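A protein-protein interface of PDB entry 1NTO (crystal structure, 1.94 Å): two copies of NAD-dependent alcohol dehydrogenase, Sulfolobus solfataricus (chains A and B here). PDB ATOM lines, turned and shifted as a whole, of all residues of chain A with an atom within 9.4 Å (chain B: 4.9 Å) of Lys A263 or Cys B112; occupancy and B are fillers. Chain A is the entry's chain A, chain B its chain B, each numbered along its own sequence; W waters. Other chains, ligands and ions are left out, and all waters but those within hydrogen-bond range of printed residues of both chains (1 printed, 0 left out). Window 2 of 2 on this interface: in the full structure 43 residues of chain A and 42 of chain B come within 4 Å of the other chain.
The side-chain amino group of Lys A263 is in hydrogen-bond range of the backbone carbonyl oxygen of Cys B112, at 3.5 Å.
The side-chain amino group of Lys A263 is in hydrogen-bond range of the backbone carbonyl oxygen of Leu B111, at 2.7 Å.
A ring nitrogen (NE2) of His B110 sits at hydrogen-bond distance from the side-chain carboxylate of Glu A288 (2.8 Å).
The side-chain hydroxyl (OH) of Tyr B103 is in hydrogen-bond range of the backbone carbonyl oxygen (O) of Lys A263 (2.8 Å).
OD1 of Asp B113 is in salt-bridge range of NZ of Lys A263 (2.7 Å).
N of Ser B114 sits close to SG of Cys B112.
The side-chain sulfur (SG) of Cys B101 sits close to the backbone NH (N) of Asp B113 (3.4 Å).
NZ of Lys A239 lies within salt-bridge range of OD1 of Asp A242.
NE2 of Gln A264 is in hydrogen-bond range of OE1 of Glu A288.
The backbone carbonyl oxygen of Val A241 lies within hydrogen-bond range of the backbone NH of Ala A262 (2.8 Å).
O of Tyr B103 sits at hydrogen-bond distance from N of Glu B108.
No position is printed for both chains.
Of the 12 pairs that touch across the chains among the printed residues, none has its exchanged pair printed and touching as well.
Printed residues of chain A that touch a printed residue of chain B: Lys A239, Ala A262, Lys A263, Gln A264, Leu A286 and Glu A288.
Among the printed residues, 12 pairs touch across the chains.
Among the printed residues, Asp or Glu carboxylates within 4 Å of a Lys or Arg side-chain nitrogen of the other chain: Lys A263 with Asp B113.
Of chain B, only Tyr B103 (2.8 Å), Leu B111 (2.7 Å), Cys B112 (3.5 Å) and Asp B113 (2.7 Å) come within 4 Å of Lys A263.
Cys B112 touches one residue of chain A.
Of chain A, only Lys A263 comes within 4 Å of Asp B113.
No residue of chain A comes within 4 Å of Ser B114.
Of the printed residues of chain A, His B110 touches Glu A288 (2.8 Å).
Of the printed residues of chain B, Ala A262 touches Tyr B103.
The nearest printed residue of chain B that does not touch Lys A263 is Ser B114 (5.6 Å).
Water W1 lies within hydrogen-bond range of O of Lys A239, N of Lys A263 and OH of Tyr B103.
Among the printed residues, pairs that only touch across the chains: Lys A239 with Tyr B103 (3.3 Å), Ala A262 with Tyr B103 (3.4 Å), Gln A264 with Tyr B103 (3.9 Å), Gln A264 with Glu B108 (3.5 Å), Gln A264 with Leu B111 (3.4 Å), Leu A286 with Leu B111 (3.998 Å) and Glu A288 with Leu B111 (3.7 Å).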
ATOM      1  N   LYS A 172      -0.779  -2.361 -11.317  1.00  0.00           N
ATOM      2  CA  LYS A 172      -0.010  -1.604 -12.323  1.00  0.00           C
ATOM      3  C   LYS A 172      -0.816  -0.863 -13.365  1.00  0.00           C
ATOM      4  O   LYS A 172      -2.008  -1.117 -13.545  1.00  0.00           O
ATOM      5  CB  LYS A 172       0.937  -2.567 -13.046  1.00  0.00           C
ATOM      6  CG  LYS A 172       2.071  -3.075 -12.157  1.00  0.00           C
ATOM      7  CD  LYS A 172       2.925  -4.122 -12.891  1.00  0.00           C
ATOM      8  CE  LYS A 172       4.162  -4.471 -12.081  1.00  0.00           C
ATOM      9  NZ  LYS A 172       5.051  -5.388 -12.857  1.00  0.00           N
ATOM     10  N   THR A 173      -0.130   0.036 -14.083  1.00  0.00           N
ATOM     11  CA  THR A 173      -0.706   0.763 -15.195  1.00  0.00           C
ATOM     12  C   THR A 173       0.173   0.551 -16.438  1.00  0.00           C
ATOM     13  O   THR A 173       1.394   0.548 -16.353  1.00  0.00           O
ATOM     14  CB  THR A 173      -0.816   2.288 -14.856  1.00  0.00           C
ATOM     15  OG1 THR A 173      -1.759   2.459 -13.783  1.00  0.00           O
ATOM     16  CG2 THR A 173      -1.304   3.076 -16.067  1.00  0.00           C
ATOM     17  N   ARG A 233       1.520  11.627 -16.047  1.00  0.00           N
ATOM     18  CA  ARG A 233       1.790  11.909 -14.648  1.00  0.00           C
ATOM     19  C   ARG A 233       0.523  12.236 -13.876  1.00  0.00           C
ATOM     20  O   ARG A 233       0.385  11.869 -12.716  1.00  0.00           O
ATOM     21  CB  ARG A 233       2.799  13.056 -14.522  1.00  0.00           C
ATOM     22  CG  ARG A 233       4.193  12.588 -14.962  1.00  0.00           C
ATOM     23  CD  ARG A 233       4.658  11.351 -14.124  1.00  0.00           C
ATOM     24  NE  ARG A 233       5.522  10.442 -14.874  1.00  0.00           N
ATOM     25  CZ  ARG A 233       6.651   9.914 -14.399  1.00  0.00           C
ATOM     26  NH1 ARG A 233       7.052  10.206 -13.170  1.00  0.00           N
ATOM     27  NH2 ARG A 233       7.389   9.098 -15.149  1.00  0.00           N
ATOM     28  N   SER A 238       1.721  10.917 -10.535  1.00  0.00           N
ATOM     29  CA  SER A 238       3.168  11.123 -10.512  1.00  0.00           C
ATOM     30  C   SER A 238       4.024   9.878 -10.441  1.00  0.00           C
ATOM     31  O   SER A 238       5.251   9.955 -10.482  1.00  0.00           O
ATOM     32  CB  SER A 238       3.523  12.078  -9.370  1.00  0.00           C
ATOM     33  OG  SER A 238       2.828  13.305  -9.567  1.00  0.00           O
ATOM     34  N   LYS A 239       3.397   8.714 -10.370  1.00  0.00           N
ATOM     35  CA  LYS A 239       4.187   7.482 -10.331  1.00  0.00           C
ATOM     36  C   LYS A 239       4.839   7.152 -11.691  1.00  0.00           C
ATOM     37  O   LYS A 239       5.979   6.653 -11.759  1.00  0.00           O
ATOM     38  CB  LYS A 239       3.306   6.300  -9.914  1.00  0.00           C
ATOM     39  CG  LYS A 239       4.114   5.026  -9.644  1.00  0.00           C
ATOM     40  CD  LYS A 239       3.224   3.785  -9.551  1.00  0.00           C
ATOM     41  CE  LYS A 239       4.075   2.530  -9.392  1.00  0.00           C
ATOM     42  NZ  LYS A 239       3.315   1.262  -9.625  1.00  0.00           N
ATOM     43  N   GLY A 240       4.111   7.437 -12.760  1.00  0.00           N
ATOM     44  CA  GLY A 240       4.500   6.985 -14.081  1.00  0.00           C
ATOM     45  C   GLY A 240       3.833   5.630 -14.306  1.00  0.00           C
ATOM     46  O   GLY A 240       3.090   5.158 -13.454  1.00  0.00           O
ATOM     47  N   VAL A 241       4.092   4.998 -15.448  1.00  0.00           N
ATOM     48  CA  VAL A 241       3.480   3.720 -15.747  1.00  0.00           C
ATOM     49  C   VAL A 241       4.436   2.561 -15.547  1.00  0.00           C
ATOM     50  O   VAL A 241       5.654   2.704 -15.709  1.00  0.00           O
ATOM     51  CB  VAL A 241       2.976   3.686 -17.182  1.00  0.00           C
ATOM     52  CG1 VAL A 241       1.872   4.737 -17.347  1.00  0.00           C
ATOM     53  CG2 VAL A 241       4.140   3.979 -18.168  1.00  0.00           C
ATOM     54  N   ASP A 242       3.881   1.398 -15.227  1.00  0.00           N
ATOM     55  CA  ASP A 242       4.709   0.242 -14.921  1.00  0.00           C
ATOM     56  C   ASP A 242       5.195  -0.475 -16.159  1.00  0.00           C
ATOM     57  O   ASP A 242       6.120  -1.293 -16.092  1.00  0.00           O
ATOM     58  CB  ASP A 242       3.928  -0.675 -13.976  1.00  0.00           C
ATOM     59  CG  ASP A 242       3.481   0.072 -12.740  1.00  0.00           C
ATOM     60  OD1 ASP A 242       4.320   0.262 -11.821  1.00  0.00           O
ATOM     61  OD2 ASP A 242       2.303   0.513 -12.701  1.00  0.00           O
ATOM     62  N   ALA A 243       4.595  -0.147 -17.308  1.00  0.00           N
ATOM     63  CA  ALA A 243       5.085  -0.703 -18.574  1.00  0.00           C
ATOM     64  C   ALA A 243       4.622   0.188 -19.706  1.00  0.00           C
ATOM     65  O   ALA A 243       3.622   0.889 -19.585  1.00  0.00           O
ATOM     66  CB  ALA A 243       4.553  -2.130 -18.803  1.00  0.00           C
ATOM     67  N   PRO A 258      10.076   6.643 -22.659  1.00  0.00           N
ATOM     68  CA  PRO A 258      10.744   6.021 -21.499  1.00  0.00           C
ATOM     69  C   PRO A 258      10.673   6.920 -20.262  1.00  0.00           C
ATOM     70  O   PRO A 258      10.744   6.445 -19.140  1.00  0.00           O
ATOM     71  CB  PRO A 258      12.184   5.826 -21.980  1.00  0.00           C
ATOM     72  CG  PRO A 258      12.010   5.562 -23.447  1.00  0.00           C
ATOM     73  CD  PRO A 258      10.930   6.579 -23.856  1.00  0.00           C
ATOM     74  N   LYS A 259      10.526   8.233 -20.481  1.00  0.00           N
ATOM     75  CA  LYS A 259      10.411   9.189 -19.389  1.00  0.00           C
ATOM     76  C   LYS A 259       9.115   9.028 -18.616  1.00  0.00           C
ATOM     77  O   LYS A 259       8.992   9.543 -17.506  1.00  0.00           O
ATOM     78  CB  LYS A 259      10.483  10.632 -19.926  1.00  0.00           C
ATOM     79  CG  LYS A 259      11.805  10.968 -20.619  1.00  0.00           C
ATOM     80  CD  LYS A 259      11.749  12.384 -21.181  1.00  0.00           C
ATOM     81  CE  LYS A 259      13.062  12.829 -21.811  1.00  0.00           C
ATOM     82  NZ  LYS A 259      12.865  14.228 -22.343  1.00  0.00           N
ATOM     83  N   ALA A 260       8.143   8.315 -19.191  1.00  0.00           N
ATOM     84  CA  ALA A 260       6.878   8.109 -18.494  1.00  0.00           C
ATOM     85  C   ALA A 260       6.963   6.900 -17.549  1.00  0.00           C
ATOM     86  O   ALA A 260       6.021   6.627 -16.811  1.00  0.00           O
ATOM     87  CB  ALA A 260       5.737   7.884 -19.515  1.00  0.00           C
ATOM     88  N   LEU A 261       8.084   6.185 -17.574  1.00  0.00           N
ATOM     89  CA  LEU A 261       8.203   4.969 -16.783  1.00  0.00           C
ATOM     90  C   LEU A 261       8.322   5.170 -15.300  1.00  0.00           C
ATOM     91  O   LEU A 261       9.087   6.015 -14.819  1.00  0.00           O
ATOM     92  CB  LEU A 261       9.408   4.146 -17.241  1.00  0.00           C
ATOM     93  CG  LEU A 261       9.337   3.515 -18.630  1.00  0.00           C
ATOM     94  CD1 LEU A 261      10.741   3.061 -19.043  1.00  0.00           C
ATOM     95  CD2 LEU A 261       8.346   2.319 -18.612  1.00  0.00           C
ATOM     96  N   ALA A 262       7.578   4.354 -14.564  1.00  0.00           N
ATOM     97  CA  ALA A 262       7.703   4.308 -13.122  1.00  0.00           C
ATOM     98  C   ALA A 262       8.978   3.517 -12.797  1.00  0.00           C
ATOM     99  O   ALA A 262       9.566   2.878 -13.676  1.00  0.00           O
ATOM    100  CB  ALA A 262       6.465   3.587 -12.518  1.00  0.00           C
ATOM    101  N   LYS A 263       9.415   3.572 -11.539  1.00  0.00           N
ATOM    102  CA  LYS A 263      10.524   2.718 -11.123  1.00  0.00           C
ATOM    103  C   LYS A 263      10.107   1.278 -11.408  1.00  0.00           C
ATOM    104  O   LYS A 263       8.929   0.918 -11.236  1.00  0.00           O
ATOM    105  CB  LYS A 263      10.827   2.925  -9.632  1.00  0.00           C
ATOM    106  CG  LYS A 263      11.593   4.250  -9.366  1.00  0.00           C
ATOM    107  CD  LYS A 263      11.705   4.601  -7.877  1.00  0.00           C
ATOM    108  CE  LYS A 263      10.395   5.264  -7.365  1.00  0.00           C
ATOM    109  NZ  LYS A 263      10.425   5.600  -5.911  1.00  0.00           N
ATOM    110  N   GLN A 264      11.078   0.481 -11.845  1.00  0.00           N
ATOM    111  CA  GLN A 264      10.901  -0.896 -12.296  1.00  0.00           C
ATOM    112  C   GLN A 264      10.051  -1.024 -13.543  1.00  0.00           C
ATOM    113  O   GLN A 264       9.706  -2.141 -13.951  1.00  0.00           O
ATOM    114  CB  GLN A 264      10.313  -1.782 -11.201  1.00  0.00           C
ATOM    115  CG  GLN A 264      11.170  -1.875  -9.972  1.00  0.00           C
ATOM    116  CD  GLN A 264      10.665  -2.954  -9.014  1.00  0.00           C
ATOM    117  OE1 GLN A 264       9.510  -2.924  -8.572  1.00  0.00           O
ATOM    118  NE2 GLN A 264      11.529  -3.908  -8.698  1.00  0.00           N
ATOM    119  N   GLY A 265       9.731   0.114 -14.155  1.00  0.00           N
ATOM    120  CA  GLY A 265       8.962   0.079 -15.375  1.00  0.00           C
ATOM    121  C   GLY A 265       9.655  -0.682 -16.492  1.00  0.00           C
ATOM    122  O   GLY A 265      10.890  -0.636 -16.626  1.00  0.00           O
ATOM    123  N   LYS A 266       8.854  -1.373 -17.307  1.00  0.00           N
ATOM    124  CA  LYS A 266       9.365  -2.108 -18.446  1.00  0.00           C
ATOM    125  C   LYS A 266       8.922  -1.450 -19.727  1.00  0.00           C
ATOM    126  O   LYS A 266       7.726  -1.240 -19.947  1.00  0.00           O
ATOM    127  CB  LYS A 266       8.863  -3.569 -18.423  1.00  0.00           C
ATOM    128  CG  LYS A 266       9.283  -4.325 -17.167  1.00  0.00           C
ATOM    129  CD  LYS A 266       8.939  -5.790 -17.250  1.00  0.00           C
ATOM    130  CE  LYS A 266       9.387  -6.507 -15.984  1.00  0.00           C
ATOM    131  NZ  LYS A 266       9.273  -8.001 -16.108  1.00  0.00           N
ATOM    132  N   LEU A 283      20.084   6.595 -15.332  1.00  0.00           N
ATOM    133  CA  LEU A 283      18.631   6.663 -15.191  1.00  0.00           C
ATOM    134  C   LEU A 283      18.075   5.242 -15.154  1.00  0.00           C
ATOM    135  O   LEU A 283      17.061   4.985 -14.503  1.00  0.00           O
ATOM    136  CB  LEU A 283      18.007   7.431 -16.363  1.00  0.00           C
ATOM    137  CG  LEU A 283      18.351   8.928 -16.499  1.00  0.00           C
ATOM    138  CD1 LEU A 283      17.805   9.496 -17.807  1.00  0.00           C
ATOM    139  CD2 LEU A 283      17.789   9.679 -15.313  1.00  0.00           C
ATOM    140  N   ILE A 284      18.742   4.325 -15.852  1.00  0.00           N
ATOM    141  CA  ILE A 284      18.300   2.931 -15.898  1.00  0.00           C
ATOM    142  C   ILE A 284      18.543   2.234 -14.568  1.00  0.00           C
ATOM    143  O   ILE A 284      17.647   1.622 -14.004  1.00  0.00           O
ATOM    144  CB  ILE A 284      19.009   2.157 -17.045  1.00  0.00           C
ATOM    145  CG1 ILE A 284      18.627   2.788 -18.384  1.00  0.00           C
ATOM    146  CG2 ILE A 284      18.594   0.656 -17.040  1.00  0.00           C
ATOM    147  CD1 ILE A 284      19.309   2.162 -19.595  1.00  0.00           C
ATOM    148  N   THR A 285      19.744   2.354 -14.029  1.00  0.00           N
ATOM    149  CA  THR A 285      20.043   1.680 -12.772  1.00  0.00           C
ATOM    150  C   THR A 285      19.320   2.306 -11.587  1.00  0.00           C
ATOM    151  O   THR A 285      18.855   1.593 -10.696  1.00  0.00           O
ATOM    152  CB  THR A 285      21.542   1.698 -12.504  1.00  0.00           C
ATOM    153  OG1 THR A 285      21.980   3.068 -12.387  1.00  0.00           O
ATOM    154  CG2 THR A 285      22.265   1.016 -13.674  1.00  0.00           C
ATOM    155  N   LEU A 286      19.199   3.628 -11.576  1.00  0.00           N
ATOM    156  CA  LEU A 286      18.553   4.273 -10.441  1.00  0.00           C
ATOM    157  C   LEU A 286      17.088   3.860 -10.301  1.00  0.00           C
ATOM    158  O   LEU A 286      16.597   3.675  -9.187  1.00  0.00           O
ATOM    159  CB  LEU A 286      18.638   5.798 -10.553  1.00  0.00           C
ATOM    160  CG  LEU A 286      19.819   6.415  -9.786  1.00  0.00           C
ATOM    161  CD1 LEU A 286      19.968   7.890 -10.135  1.00  0.00           C
ATOM    162  CD2 LEU A 286      19.581   6.266  -8.289  1.00  0.00           C
ATOM    163  N   SER A 287      16.400   3.712 -11.429  1.00  0.00           N
ATOM    164  CA  SER A 287      14.971   3.376 -11.413  1.00  0.00           C
ATOM    165  C   SER A 287      14.684   1.893 -11.666  1.00  0.00           C
ATOM    166  O   SER A 287      13.512   1.459 -11.635  1.00  0.00           O
ATOM    167  CB  SER A 287      14.253   4.202 -12.475  1.00  0.00           C
ATOM    168  OG  SER A 287      14.227   5.560 -12.091  1.00  0.00           O
ATOM    169  N   GLU A 288      15.745   1.129 -11.908  1.00  0.00           N
ATOM    170  CA  GLU A 288      15.632  -0.284 -12.250  1.00  0.00           C
ATOM    171  C   GLU A 288      14.695  -0.463 -13.437  1.00  0.00           C
ATOM    172  O   GLU A 288      13.919  -1.412 -13.492  1.00  0.00           O
ATOM    173  CB  GLU A 288      15.112  -1.132 -11.070  1.00  0.00           C
ATOM    174  CG  GLU A 288      16.106  -1.271  -9.894  1.00  0.00           C
ATOM    175  CD  GLU A 288      15.820  -2.466  -8.968  1.00  0.00           C
ATOM    176  OE1 GLU A 288      14.865  -3.239  -9.232  1.00  0.00           O
ATOM    177  OE2 GLU A 288      16.573  -2.648  -7.976  1.00  0.00           O
ATOM    178  N   ILE A 289      14.759   0.425 -14.413  1.00  0.00           N
ATOM    179  CA  ILE A 289      13.885   0.171 -15.538  1.00  0.00           C
ATOM    180  C   ILE A 289      14.504  -0.872 -16.459  1.00  0.00           C
ATOM    181  O   ILE A 289      15.692  -1.223 -16.319  1.00  0.00           O
ATOM    182  CB  ILE A 289      13.539   1.451 -16.289  1.00  0.00           C
ATOM    183  CG1 ILE A 289      14.789   2.090 -16.841  1.00  0.00           C
ATOM    184  CG2 ILE A 289      12.792   2.400 -15.346  1.00  0.00           C
ATOM    185  CD1 ILE A 289      14.498   3.375 -17.582  1.00  0.00           C
ATOM    186  N   GLN A 290      13.690  -1.392 -17.368  1.00  0.00           N
ATOM    187  CA  GLN A 290      14.115  -2.416 -18.297  1.00  0.00           C
ATOM    188  C   GLN A 290      13.637  -2.021 -19.678  1.00  0.00           C
ATOM    189  O   GLN A 290      12.514  -1.552 -19.835  1.00  0.00           O
ATOM    190  CB  GLN A 290      13.493  -3.780 -17.955  1.00  0.00           C
ATOM    191  CG  GLN A 290      13.838  -4.288 -16.578  1.00  0.00           C
ATOM    192  CD  GLN A 290      13.239  -5.646 -16.252  1.00  0.00           C
ATOM    193  OE1 GLN A 290      12.852  -6.406 -17.131  1.00  0.00           O
ATOM    194  NE2 GLN A 290      13.188  -5.958 -14.974  1.00  0.00           N
ATOM    195  N   GLN B  96      16.542   1.723   3.410  1.00  0.00           N
ATOM    196  CA  GLN B  96      15.270   1.589   4.115  1.00  0.00           C
ATOM    197  C   GLN B  96      14.137   2.428   3.560  1.00  0.00           C
ATOM    198  O   GLN B  96      14.337   3.585   3.164  1.00  0.00           O
ATOM    199  CB  GLN B  96      15.479   1.910   5.613  1.00  0.00           C
ATOM    200  CG  GLN B  96      16.439   0.954   6.268  1.00  0.00           C
ATOM    201  CD  GLN B  96      16.903   1.364   7.659  1.00  0.00           C
ATOM    202  OE1 GLN B  96      16.235   2.121   8.363  1.00  0.00           O
ATOM    203  NE2 GLN B  96      18.047   0.828   8.071  1.00  0.00           N
ATOM    204  N   GLY B  97      12.946   1.827   3.539  1.00  0.00           N
ATOM    205  CA  GLY B  97      11.762   2.508   3.044  1.00  0.00           C
ATOM    206  C   GLY B  97      10.843   2.903   4.189  1.00  0.00           C
ATOM    207  O   GLY B  97      10.987   2.413   5.305  1.00  0.00           O
ATOM    208  N   GLU B  98       9.893   3.787   3.915  1.00  0.00           N
ATOM    209  CA  GLU B  98       8.990   4.279   4.949  1.00  0.00           C
ATOM    210  C   GLU B  98       7.743   3.389   5.139  1.00  0.00           C
ATOM    211  O   GLU B  98       7.039   3.517   6.136  1.00  0.00           O
ATOM    212  CB  GLU B  98       8.602   5.728   4.635  1.00  0.00           C
ATOM    213  CG  GLU B  98       8.146   5.993   3.180  1.00  0.00           C
ATOM    214  CD  GLU B  98       6.849   5.269   2.827  1.00  0.00           C
ATOM    215  OE1 GLU B  98       5.851   5.480   3.550  1.00  0.00           O
ATOM    216  OE2 GLU B  98       6.812   4.492   1.831  1.00  0.00           O
ATOM    217  N   CYS B 101       4.445   3.677   0.566  1.00  0.00           N
ATOM    218  CA  CYS B 101       4.399   3.838  -0.887  1.00  0.00           C
ATOM    219  C   CYS B 101       4.264   2.497  -1.605  1.00  0.00           C
ATOM    220  O   CYS B 101       4.385   1.440  -1.001  1.00  0.00           O
ATOM    221  CB  CYS B 101       5.644   4.580  -1.412  1.00  0.00           C
ATOM    222  SG  CYS B 101       7.189   3.585  -1.481  1.00  0.00           S
ATOM    223  N   TYR B 103       6.215   0.921  -3.677  1.00  0.00           N
ATOM    224  CA  TYR B 103       7.401   0.081  -3.643  1.00  0.00           C
ATOM    225  C   TYR B 103       7.629  -0.586  -2.318  1.00  0.00           C
ATOM    226  O   TYR B 103       8.107  -1.722  -2.268  1.00  0.00           O
ATOM    227  CB  TYR B 103       8.614   0.918  -4.077  1.00  0.00           C
ATOM    228  CG  TYR B 103       8.441   1.342  -5.514  1.00  0.00           C
ATOM    229  CD1 TYR B 103       8.697   0.452  -6.559  1.00  0.00           C
ATOM    230  CD2 TYR B 103       7.866   2.567  -5.824  1.00  0.00           C
ATOM    231  CE1 TYR B 103       8.361   0.778  -7.890  1.00  0.00           C
ATOM    232  CE2 TYR B 103       7.524   2.899  -7.130  1.00  0.00           C
ATOM    233  CZ  TYR B 103       7.769   2.003  -8.159  1.00  0.00           C
ATOM    234  OH  TYR B 103       7.382   2.335  -9.443  1.00  0.00           O
ATOM    235  N   CYS B 104       7.295   0.091  -1.225  1.00  0.00           N
ATOM    236  CA  CYS B 104       7.431  -0.558   0.081  1.00  0.00           C
ATOM    237  C   CYS B 104       6.365  -1.660   0.217  1.00  0.00           C
ATOM    238  O   CYS B 104       6.623  -2.732   0.757  1.00  0.00           O
ATOM    239  CB  CYS B 104       7.287   0.483   1.209  1.00  0.00           C
ATOM    240  SG  CYS B 104       8.754   1.581   1.354  1.00  0.00           S
ATOM    241  N   GLU B 108       9.780  -3.912  -2.298  1.00  0.00           N
ATOM    242  CA  GLU B 108      10.974  -3.384  -2.971  1.00  0.00           C
ATOM    243  C   GLU B 108      11.344  -2.081  -2.249  1.00  0.00           C
ATOM    244  O   GLU B 108      11.349  -1.020  -2.862  1.00  0.00           O
ATOM    245  CB  GLU B 108      10.680  -3.095  -4.446  1.00  0.00           C
ATOM    246  CG  GLU B 108      10.259  -4.320  -5.239  1.00  0.00           C
ATOM    247  CD  GLU B 108      11.397  -5.318  -5.472  1.00  0.00           C
ATOM    248  OE1 GLU B 108      12.534  -5.107  -5.002  1.00  0.00           O
ATOM    249  OE2 GLU B 108      11.143  -6.331  -6.136  1.00  0.00           O
ATOM    250  N   GLU B 109      11.662  -2.184  -0.951  1.00  0.00           N
ATOM    251  CA  GLU B 109      11.873  -0.993  -0.100  1.00  0.00           C
ATOM    252  C   GLU B 109      12.997  -0.052  -0.534  1.00  0.00           C
ATOM    253  O   GLU B 109      12.947   1.151  -0.253  1.00  0.00           O
ATOM    254  CB  GLU B 109      12.130  -1.409   1.366  1.00  0.00           C
ATOM    255  N   HIS B 110      14.015  -0.588  -1.192  1.00  0.00           N
ATOM    256  CA  HIS B 110      15.136   0.251  -1.603  1.00  0.00           C
ATOM    257  C   HIS B 110      14.666   1.243  -2.652  1.00  0.00           C
ATOM    258  O   HIS B 110      15.308   2.269  -2.869  1.00  0.00           O
ATOM    259  CB  HIS B 110      16.274  -0.603  -2.165  1.00  0.00           C
ATOM    260  CG  HIS B 110      15.881  -1.425  -3.357  1.00  0.00           C
ATOM    261  ND1 HIS B 110      14.866  -2.361  -3.312  1.00  0.00           N
ATOM    262  CD2 HIS B 110      16.394  -1.481  -4.611  1.00  0.00           C
ATOM    263  CE1 HIS B 110      14.775  -2.964  -4.486  1.00  0.00           C
ATOM    264  NE2 HIS B 110      15.695  -2.452  -5.292  1.00  0.00           N
ATOM    265  N   LEU B 111      13.535   0.952  -3.303  1.00  0.00           N
ATOM    266  CA  LEU B 111      13.008   1.861  -4.331  1.00  0.00           C
ATOM    267  C   LEU B 111      11.910   2.779  -3.782  1.00  0.00           C
ATOM    268  O   LEU B 111      11.144   3.376  -4.535  1.00  0.00           O
ATOM    269  CB  LEU B 111      12.478   1.052  -5.533  1.00  0.00           C
ATOM    270  CG  LEU B 111      13.545   0.189  -6.220  1.00  0.00           C
ATOM    271  CD1 LEU B 111      12.926  -0.700  -7.308  1.00  0.00           C
ATOM    272  CD2 LEU B 111      14.595   1.134  -6.837  1.00  0.00           C
ATOM    273  N   CYS B 112      11.869   2.898  -2.459  1.00  0.00           N
ATOM    274  CA  CYS B 112      10.882   3.719  -1.766  1.00  0.00           C
ATOM    275  C   CYS B 112      10.831   5.128  -2.352  1.00  0.00           C
ATOM    276  O   CYS B 112      11.867   5.679  -2.761  1.00  0.00           O
ATOM    277  CB  CYS B 112      11.242   3.757  -0.280  1.00  0.00           C
ATOM    278  SG  CYS B 112      10.221   4.860   0.740  1.00  0.00           S
ATOM    279  N   ASP B 113       9.633   5.711  -2.390  1.00  0.00           N
ATOM    280  CA  ASP B 113       9.430   7.066  -2.897  1.00  0.00           C
ATOM    281  C   ASP B 113      10.040   8.122  -1.960  1.00  0.00           C
ATOM    282  O   ASP B 113      10.301   9.240  -2.370  1.00  0.00           O
ATOM    283  CB  ASP B 113       7.935   7.380  -3.019  1.00  0.00           C
ATOM    284  CG  ASP B 113       7.257   6.621  -4.138  1.00  0.00           C
ATOM    285  OD1 ASP B 113       7.959   6.085  -5.027  1.00  0.00           O
ATOM    286  OD2 ASP B 113       6.012   6.586  -4.133  1.00  0.00           O
ATOM    287  N   SER B 114      10.238   7.751  -0.705  1.00  0.00           N
ATOM    288  CA  SER B 114      10.776   8.667   0.310  1.00  0.00           C
ATOM    289  C   SER B 114      11.769   7.840   1.070  1.00  0.00           C
ATOM    290  O   SER B 114      11.564   7.520   2.246  1.00  0.00           O
ATOM    291  CB  SER B 114       9.645   9.129   1.238  1.00  0.00           C
ATOM    292  OG  SER B 114       8.657   9.832   0.484  1.00  0.00           O
ATOM    293  N   PRO B 115      12.870   7.470   0.409  1.00  0.00           N
ATOM    294  CA  PRO B 115      13.880   6.607   1.018  1.00  0.00           C
ATOM    295  C   PRO B 115      14.578   7.179   2.249  1.00  0.00           C
ATOM    296  O   PRO B 115      14.771   8.394   2.371  1.00  0.00           O
ATOM    297  CB  PRO B 115      14.851   6.363  -0.124  1.00  0.00           C
ATOM    298  CG  PRO B 115      14.806   7.652  -0.860  1.00  0.00           C
ATOM    299  CD  PRO B 115      13.337   8.000  -0.882  1.00  0.00           C
HETATM  300  O   HOH W   1       7.972   5.722  -9.826  1.00  0.00           O
